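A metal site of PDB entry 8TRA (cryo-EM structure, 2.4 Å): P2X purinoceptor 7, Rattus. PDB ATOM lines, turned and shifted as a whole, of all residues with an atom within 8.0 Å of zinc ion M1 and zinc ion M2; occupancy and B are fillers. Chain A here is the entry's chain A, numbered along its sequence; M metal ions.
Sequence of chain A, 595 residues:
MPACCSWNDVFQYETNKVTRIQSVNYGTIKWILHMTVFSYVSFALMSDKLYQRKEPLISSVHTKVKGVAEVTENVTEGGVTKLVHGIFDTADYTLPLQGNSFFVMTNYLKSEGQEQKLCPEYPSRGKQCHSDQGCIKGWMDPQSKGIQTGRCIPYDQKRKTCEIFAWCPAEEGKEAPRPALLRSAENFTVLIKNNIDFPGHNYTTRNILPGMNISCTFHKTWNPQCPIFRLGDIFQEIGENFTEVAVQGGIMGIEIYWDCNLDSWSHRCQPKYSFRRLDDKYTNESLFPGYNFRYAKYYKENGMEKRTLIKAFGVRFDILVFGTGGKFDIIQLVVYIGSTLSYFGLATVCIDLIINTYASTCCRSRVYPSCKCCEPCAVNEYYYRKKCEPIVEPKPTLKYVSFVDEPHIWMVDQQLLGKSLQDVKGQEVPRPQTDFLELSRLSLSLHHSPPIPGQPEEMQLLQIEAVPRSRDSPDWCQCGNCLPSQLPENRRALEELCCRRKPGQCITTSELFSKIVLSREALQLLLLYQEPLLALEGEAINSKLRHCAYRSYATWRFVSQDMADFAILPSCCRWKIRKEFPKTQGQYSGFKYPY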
ATOM      1  N   VAL A 404      23.984  10.653  33.238  1.00  0.00           N
ATOM      2  CA  VAL A 404      23.416  10.243  34.523  1.00  0.00           C
ATOM      3  C   VAL A 404      24.088   8.979  35.025  1.00  0.00           C
ATOM      4  O   VAL A 404      24.327   8.828  36.235  1.00  0.00           O
ATOM      5  CB  VAL A 404      21.887  10.069  34.395  1.00  0.00           C
ATOM      6  CG1 VAL A 404      21.554   8.774  33.658  1.00  0.00           C
ATOM      7  CG2 VAL A 404      21.236  10.090  35.774  1.00  0.00           C
ATOM      8  N   GLN A 422      27.862  12.777  21.306  1.00  0.00           N
ATOM      9  CA  GLN A 422      27.842  11.578  22.128  1.00  0.00           C
ATOM     10  C   GLN A 422      29.032  10.677  21.833  1.00  0.00           C
ATOM     11  O   GLN A 422      29.658  10.131  22.743  1.00  0.00           O
ATOM     12  CB  GLN A 422      26.528  10.829  21.924  1.00  0.00           C
ATOM     13  CG  GLN A 422      26.310   9.668  22.883  1.00  0.00           C
ATOM     14  CD  GLN A 422      25.537  10.065  24.132  1.00  0.00           C
ATOM     15  OE1 GLN A 422      25.126  11.218  24.273  1.00  0.00           O
ATOM     16  NE2 GLN A 422      25.340   9.121  25.034  1.00  0.00           N
ATOM     17  N   SER A 473      14.195   5.372  18.273  1.00  0.00           N
ATOM     18  CA  SER A 473      15.088   6.413  18.761  1.00  0.00           C
ATOM     19  C   SER A 473      16.351   6.466  17.903  1.00  0.00           C
ATOM     20  O   SER A 473      16.734   5.476  17.276  1.00  0.00           O
ATOM     21  CB  SER A 473      15.446   6.168  20.220  1.00  0.00           C
ATOM     22  OG  SER A 473      16.368   5.089  20.345  1.00  0.00           O
ATOM     23  N   PRO A 474      17.029   7.614  17.866  1.00  0.00           N
ATOM     24  CA  PRO A 474      18.267   7.708  17.098  1.00  0.00           C
ATOM     25  C   PRO A 474      19.292   6.673  17.535  1.00  0.00           C
ATOM     26  O   PRO A 474      19.204   6.077  18.620  1.00  0.00           O
ATOM     27  CB  PRO A 474      18.763   9.139  17.386  1.00  0.00           C
ATOM     28  CG  PRO A 474      17.555   9.896  17.780  1.00  0.00           C
ATOM     29  CD  PRO A 474      16.590   8.918  18.401  1.00  0.00           C
ATOM     30  N   TRP A 476      22.450   7.119  18.335  1.00  0.00           N
ATOM     31  CA  TRP A 476      23.256   7.578  19.458  1.00  0.00           C
ATOM     32  C   TRP A 476      22.468   7.676  20.765  1.00  0.00           C
ATOM     33  O   TRP A 476      23.075   7.807  21.823  1.00  0.00           O
ATOM     34  CB  TRP A 476      23.889   8.945  19.153  1.00  0.00           C
ATOM     35  CG  TRP A 476      22.941   9.956  18.576  1.00  0.00           C
ATOM     36  CD1 TRP A 476      22.827  10.318  17.273  1.00  0.00           C
ATOM     37  CD2 TRP A 476      21.982  10.737  19.301  1.00  0.00           C
ATOM     38  NE1 TRP A 476      21.857  11.274  17.132  1.00  0.00           N
ATOM     39  CE2 TRP A 476      21.319  11.553  18.358  1.00  0.00           C
ATOM     40  CE3 TRP A 476      21.610  10.826  20.638  1.00  0.00           C
ATOM     41  CZ2 TRP A 476      20.310  12.437  18.718  1.00  0.00           C
ATOM     42  CZ3 TRP A 476      20.610  11.714  20.998  1.00  0.00           C
ATOM     43  CH2 TRP A 476      19.974  12.509  20.044  1.00  0.00           C
ATOM     44  N   CYS A 477      21.142   7.615  20.702  1.00  0.00           N
ATOM     45  CA  CYS A 477      20.324   7.706  21.908  1.00  0.00           C
ATOM     46  C   CYS A 477      20.326   6.376  22.654  1.00  0.00           C
ATOM     47  O   CYS A 477      20.241   5.308  22.050  1.00  0.00           O
ATOM     48  CB  CYS A 477      18.896   8.108  21.558  1.00  0.00           C
ATOM     49  SG  CYS A 477      17.766   8.086  22.964  1.00  0.00           S
ATOM     50  N   GLN A 478      20.407   6.463  23.986  1.00  0.00           N
ATOM     51  CA  GLN A 478      20.362   5.295  24.858  1.00  0.00           C
ATOM     52  C   GLN A 478      19.263   5.419  25.904  1.00  0.00           C
ATOM     53  O   GLN A 478      19.295   4.724  26.925  1.00  0.00           O
ATOM     54  CB  GLN A 478      21.722   5.079  25.525  1.00  0.00           C
ATOM     55  CG  GLN A 478      22.694   4.234  24.721  1.00  0.00           C
ATOM     56  CD  GLN A 478      23.837   5.058  24.136  1.00  0.00           C
ATOM     57  OE1 GLN A 478      24.345   5.970  24.782  1.00  0.00           O
ATOM     58  NE2 GLN A 478      24.246   4.725  22.920  1.00  0.00           N
ATOM     59  N   CYS A 479      18.281   6.286  25.674  1.00  0.00           N
ATOM     60  CA  CYS A 479      17.195   6.506  26.624  1.00  0.00           C
ATOM     61  C   CYS A 479      15.803   6.441  26.014  1.00  0.00           C
ATOM     62  O   CYS A 479      14.832   6.327  26.763  1.00  0.00           O
ATOM     63  CB  CYS A 479      17.368   7.862  27.318  1.00  0.00           C
ATOM     64  SG  CYS A 479      16.721   9.270  26.388  1.00  0.00           S
ATOM     65  N   GLY A 480      15.677   6.498  24.692  1.00  0.00           N
ATOM     66  CA  GLY A 480      14.386   6.361  24.037  1.00  0.00           C
ATOM     67  C   GLY A 480      13.538   7.607  24.010  1.00  0.00           C
ATOM     68  O   GLY A 480      12.398   7.554  23.535  1.00  0.00           O
ATOM     69  N   ASN A 481      14.055   8.739  24.505  1.00  0.00           N
ATOM     70  CA  ASN A 481      13.296   9.987  24.528  1.00  0.00           C
ATOM     71  C   ASN A 481      13.946  11.095  23.704  1.00  0.00           C
ATOM     72  O   ASN A 481      13.360  12.173  23.567  1.00  0.00           O
ATOM     73  CB  ASN A 481      13.116  10.473  25.972  1.00  0.00           C
ATOM     74  CG  ASN A 481      12.383   9.475  26.834  1.00  0.00           C
ATOM     75  OD1 ASN A 481      12.968   8.806  27.683  1.00  0.00           O
ATOM     76  ND2 ASN A 481      11.070   9.359  26.620  1.00  0.00           N
ATOM     77  N   CYS A 482      15.141  10.866  23.163  1.00  0.00           N
ATOM     78  CA  CYS A 482      15.814  11.874  22.360  1.00  0.00           C
ATOM     79  C   CYS A 482      15.220  11.918  20.959  1.00  0.00           C
ATOM     80  O   CYS A 482      14.616  10.960  20.467  1.00  0.00           O
ATOM     81  CB  CYS A 482      17.309  11.586  22.290  1.00  0.00           C
ATOM     82  SG  CYS A 482      18.171  11.753  23.867  1.00  0.00           S
ATOM     83  N   LEU A 483      15.401  13.063  20.300  1.00  0.00           N
ATOM     84  CA  LEU A 483      14.908  13.310  18.957  1.00  0.00           C
ATOM     85  C   LEU A 483      16.006  13.921  18.108  1.00  0.00           C
ATOM     86  O   LEU A 483      16.947  14.522  18.641  1.00  0.00           O
ATOM     87  CB  LEU A 483      13.698  14.250  18.991  1.00  0.00           C
ATOM     88  CG  LEU A 483      12.561  13.863  19.944  1.00  0.00           C
ATOM     89  CD1 LEU A 483      11.594  15.019  20.116  1.00  0.00           C
ATOM     90  CD2 LEU A 483      11.844  12.625  19.436  1.00  0.00           C
ATOM     91  N   LEU A 497      23.205  14.461  21.441  1.00  0.00           N
ATOM     92  CA  LEU A 497      23.689  14.028  22.737  1.00  0.00           C
ATOM     93  C   LEU A 497      22.543  13.414  23.527  1.00  0.00           C
ATOM     94  O   LEU A 497      21.413  13.914  23.495  1.00  0.00           O
ATOM     95  CB  LEU A 497      24.285  15.206  23.519  1.00  0.00           C
ATOM     96  CG  LEU A 497      24.804  14.937  24.933  1.00  0.00           C
ATOM     97  CD1 LEU A 497      26.185  14.318  24.886  1.00  0.00           C
ATOM     98  CD2 LEU A 497      24.811  16.224  25.745  1.00  0.00           C
ATOM     99  N   CYS A 498      22.834  12.321  24.221  1.00  0.00           N
ATOM    100  CA  CYS A 498      21.868  11.619  25.058  1.00  0.00           C
ATOM    101  C   CYS A 498      22.216  11.813  26.532  1.00  0.00           C
ATOM    102  O   CYS A 498      23.336  12.186  26.880  1.00  0.00           O
ATOM    103  CB  CYS A 498      21.829  10.126  24.718  1.00  0.00           C
ATOM    104  SG  CYS A 498      20.440   9.233  25.472  1.00  0.00           S
ATOM    105  N   CYS A 499      21.227  11.556  27.380  1.00  0.00           N
ATOM    106  CA  CYS A 499      21.412  11.721  28.825  1.00  0.00           C
ATOM    107  C   CYS A 499      22.308  10.653  29.441  1.00  0.00           C
ATOM    108  O   CYS A 499      22.708  10.810  30.598  1.00  0.00           O
ATOM    109  CB  CYS A 499      20.059  11.701  29.523  1.00  0.00           C
ATOM    110  SG  CYS A 499      19.089  10.200  29.231  1.00  0.00           S
ATOM    111  N   ARG A 500      22.648   9.595  28.699  1.00  0.00           N
ATOM    112  CA  ARG A 500      23.437   8.511  29.250  1.00  0.00           C
ATOM    113  C   ARG A 500      24.277   7.885  28.149  1.00  0.00           C
ATOM    114  O   ARG A 500      24.006   8.045  26.956  1.00  0.00           O
ATOM    115  CB  ARG A 500      22.546   7.439  29.891  1.00  0.00           C
ATOM    116  CG  ARG A 500      21.309   7.081  29.085  1.00  0.00           C
ATOM    117  CD  ARG A 500      20.386   6.153  29.853  1.00  0.00           C
ATOM    118  NE  ARG A 500      21.113   5.296  30.788  1.00  0.00           N
ATOM    119  CZ  ARG A 500      20.753   5.054  32.042  1.00  0.00           C
ATOM    120  NH1 ARG A 500      19.644   5.568  32.561  1.00  0.00           N
ATOM    121  NH2 ARG A 500      21.518   4.281  32.799  1.00  0.00           N
ATOM    122  N   GLY A 504      19.229   2.572  29.264  1.00  0.00           N
ATOM    123  CA  GLY A 504      18.639   2.644  30.586  1.00  0.00           C
ATOM    124  C   GLY A 504      17.499   3.630  30.612  1.00  0.00           C
ATOM    125  O   GLY A 504      16.971   4.022  29.574  1.00  0.00           O
ATOM    126  N   GLN A 505      17.121   4.034  31.826  1.00  0.00           N
ATOM    127  CA  GLN A 505      16.015   4.963  32.008  1.00  0.00           C
ATOM    128  C   GLN A 505      16.493   6.402  31.848  1.00  0.00           C
ATOM    129  O   GLN A 505      17.576   6.770  32.322  1.00  0.00           O
ATOM    130  CB  GLN A 505      15.378   4.772  33.388  1.00  0.00           C
ATOM    131  CG  GLN A 505      16.365   4.698  34.535  1.00  0.00           C
ATOM    132  CD  GLN A 505      15.717   4.967  35.883  1.00  0.00           C
ATOM    133  OE1 GLN A 505      14.614   5.516  35.963  1.00  0.00           O
ATOM    134  NE2 GLN A 505      16.395   4.577  36.952  1.00  0.00           N
ATOM    135  N   CYS A 506      15.684   7.210  31.183  1.00  0.00           N
ATOM    136  CA  CYS A 506      16.021   8.607  30.957  1.00  0.00           C
ATOM    137  C   CYS A 506      16.007   9.391  32.263  1.00  0.00           C
ATOM    138  O   CYS A 506      15.240   9.089  33.183  1.00  0.00           O
ATOM    139  CB  CYS A 506      15.052   9.240  29.956  1.00  0.00           C
ATOM    140  SG  CYS A 506      15.394  10.968  29.564  1.00  0.00           S
ATOM    141  N   ILE A 507      16.865  10.402  32.333  1.00  0.00           N
ATOM    142  CA  ILE A 507      16.910  11.259  33.514  1.00  0.00           C
ATOM    143  C   ILE A 507      15.590  11.998  33.694  1.00  0.00           C
ATOM    144  O   ILE A 507      15.229  12.382  34.817  1.00  0.00           O
ATOM    145  CB  ILE A 507      18.097  12.243  33.425  1.00  0.00           C
ATOM    146  CG1 ILE A 507      18.301  12.947  34.765  1.00  0.00           C
ATOM    147  CG2 ILE A 507      17.860  13.261  32.321  1.00  0.00           C
ATOM    148  CD1 ILE A 507      19.620  13.678  34.866  1.00  0.00           C
ATOM    149  N   THR A 508      14.859  12.212  32.602  1.00  0.00           N
ATOM    150  CA  THR A 508      13.582  12.916  32.690  1.00  0.00           C
ATOM    151  C   THR A 508      12.588  12.150  33.560  1.00  0.00           C
ATOM    152  O   THR A 508      11.689  12.760  34.154  1.00  0.00           O
ATOM    153  CB  THR A 508      12.991  13.125  31.303  1.00  0.00           C
ATOM    154  OG1 THR A 508      12.814  11.863  30.650  1.00  0.00           O
ATOM    155  CG2 THR A 508      13.909  14.008  30.457  1.00  0.00           C
ATOM    156  N   THR A 509      12.731  10.823  33.654  1.00  0.00           N
ATOM    157  CA  THR A 509      11.801  10.029  34.452  1.00  0.00           C
ATOM    158  C   THR A 509      11.878  10.382  35.937  1.00  0.00           C
ATOM    159  O   THR A 509      10.899  10.152  36.657  1.00  0.00           O
ATOM    160  CB  THR A 509      12.092   8.541  34.266  1.00  0.00           C
ATOM    161  OG1 THR A 509      13.383   8.225  34.778  1.00  0.00           O
ATOM    162  CG2 THR A 509      12.030   8.174  32.789  1.00  0.00           C
ATOM    163  N   PHE A 513      13.525  16.073  37.972  1.00  0.00           N
ATOM    164  CA  PHE A 513      13.497  16.768  36.690  1.00  0.00           C
ATOM    165  C   PHE A 513      12.260  17.644  36.563  1.00  0.00           C
ATOM    166  O   PHE A 513      12.346  18.798  36.134  1.00  0.00           O
ATOM    167  CB  PHE A 513      13.565  15.765  35.538  1.00  0.00           C
ATOM    168  CG  PHE A 513      13.742  16.392  34.192  1.00  0.00           C
ATOM    169  CD1 PHE A 513      12.644  16.864  33.484  1.00  0.00           C
ATOM    170  CD2 PHE A 513      14.996  16.539  33.636  1.00  0.00           C
ATOM    171  CE1 PHE A 513      12.804  17.446  32.240  1.00  0.00           C
ATOM    172  CE2 PHE A 513      15.159  17.113  32.396  1.00  0.00           C
ATOM    173  CZ  PHE A 513      14.065  17.576  31.694  1.00  0.00           C
ATOM    174  N   TYR A 553      18.670  23.040  34.729  1.00  0.00           N
ATOM    175  CA  TYR A 553      19.251  21.735  34.441  1.00  0.00           C
ATOM    176  C   TYR A 553      20.776  21.811  34.440  1.00  0.00           C
ATOM    177  O   TYR A 553      21.448  20.928  34.977  1.00  0.00           O
ATOM    178  CB  TYR A 553      18.739  21.206  33.102  1.00  0.00           C
ATOM    179  CG  TYR A 553      19.399  19.909  32.690  1.00  0.00           C
ATOM    180  CD1 TYR A 553      18.888  18.681  33.076  1.00  0.00           C
ATOM    181  CD2 TYR A 553      20.548  19.914  31.907  1.00  0.00           C
ATOM    182  CE1 TYR A 553      19.484  17.501  32.699  1.00  0.00           C
ATOM    183  CE2 TYR A 553      21.162  18.740  31.529  1.00  0.00           C
ATOM    184  CZ  TYR A 553      20.625  17.532  31.926  1.00  0.00           C
ATOM    185  OH  TYR A 553      21.230  16.359  31.557  1.00  0.00           O
ATOM    186  N   PRO A 570      21.093  17.414  27.021  1.00  0.00           N
ATOM    187  CA  PRO A 570      20.730  16.253  26.199  1.00  0.00           C
ATOM    188  C   PRO A 570      19.494  16.551  25.360  1.00  0.00           C
ATOM    189  O   PRO A 570      18.656  17.387  25.712  1.00  0.00           O
ATOM    190  CB  PRO A 570      20.459  15.148  27.227  1.00  0.00           C
ATOM    191  CG  PRO A 570      21.142  15.603  28.470  1.00  0.00           C
ATOM    192  CD  PRO A 570      21.074  17.087  28.455  1.00  0.00           C
ATOM    193  N   SER A 571      19.389  15.836  24.236  1.00  0.00           N
ATOM    194  CA  SER A 571      18.259  16.050  23.347  1.00  0.00           C
ATOM    195  C   SER A 571      16.940  15.750  24.038  1.00  0.00           C
ATOM    196  O   SER A 571      15.953  16.484  23.856  1.00  0.00           O
ATOM    197  CB  SER A 571      18.408  15.188  22.091  1.00  0.00           C
ATOM    198  OG  SER A 571      17.349  15.404  21.182  1.00  0.00           O
ATOM    199  N   CYS A 572      16.896  14.688  24.841  1.00  0.00           N
ATOM    200  CA  CYS A 572      15.658  14.334  25.532  1.00  0.00           C
ATOM    201  C   CYS A 572      15.197  15.465  26.443  1.00  0.00           C
ATOM    202  O   CYS A 572      14.046  15.915  26.357  1.00  0.00           O
ATOM    203  CB  CYS A 572      15.862  13.055  26.342  1.00  0.00           C
ATOM    204  SG  CYS A 572      17.515  12.901  27.074  1.00  0.00           S
ATOM    205  N   CYS A 573      16.086  15.949  27.319  1.00  0.00           N
ATOM    206  CA  CYS A 573      15.715  17.001  28.243  1.00  0.00           C
ATOM    207  C   CYS A 573      15.418  18.304  27.516  1.00  0.00           C
ATOM    208  O   CYS A 573      14.470  19.015  27.849  1.00  0.00           O
ATOM    209  CB  CYS A 573      16.823  17.206  29.271  1.00  0.00           C
ATOM    210  SG  CYS A 573      17.455  15.672  29.984  1.00  0.00           S
HETATM  211 ZN    ZN M   1      18.279   9.576  24.686  1.00  0.00          ZN
HETATM  212 ZN    ZN M   2      17.178  10.821  28.063  1.00  0.00          ZN
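Zinc ion M1 is bound by the side-chain sulfur (SG) of Cys 498, the side-chain sulfur (SG) of Cys 479, the side-chain sulfur (SG) of Cys 482 and the side-chain sulfur (SG) of Cys 477.
Zinc ion M1 has four donor atoms within binding distance.
Residues that only touch zinc ion M1: Gln 478 (3.8 Å).
Of the 28 residues printed, 5 come within 4 Å of zinc ion M1.
Along chain A the residues within 4 Å of zinc ion M1 span positions 477 to 498.
The nearest printed residue that does not touch zinc ion M1 is Gly 480 (4.03 Å).
Zinc ion M2 is bound by SG of Cys 499, SG of Cys 572, SG of Cys 479 and SG of Cys 506.
The nearest printed residue that does not touch zinc ion M2 is Ile 507 (4.3 Å).
The backbone NH of Gln 478 lies close to the side-chain sulfur of Cys 498, at 3.1 Å.
OE1 of Gln 422 sits at hydrogen-bond distance from N of Cys 498, at 2.5 Å.
The side-chain sulfur (SG) of Cys 482 sits close to the backbone NH (N) of Cys 572 (3.3 Å).
The side-chain sulfur (SG) of Cys 506 sits close to the side-chain amide oxygen (OD1) of Asn 481 (3.8 Å).
The side-chain hydroxyl (OG1) of Thr 508 sits close to the side-chain sulfur (SG) of Cys 506, 2.9 Å away.
The side-chain amide nitrogen of Gln 478 lies within hydrogen-bond range of the backbone carbonyl oxygen of Trp 476 (3.5 Å).
The backbone carbonyl oxygen (O) of Gln 478 is in hydrogen-bond range of the backbone NH (N) of Gly 504 (3.2 Å).
The side-chain amide nitrogen of Gln 422 lies within hydrogen-bond range of the side-chain amide oxygen of Gln 478 (3.3 Å).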
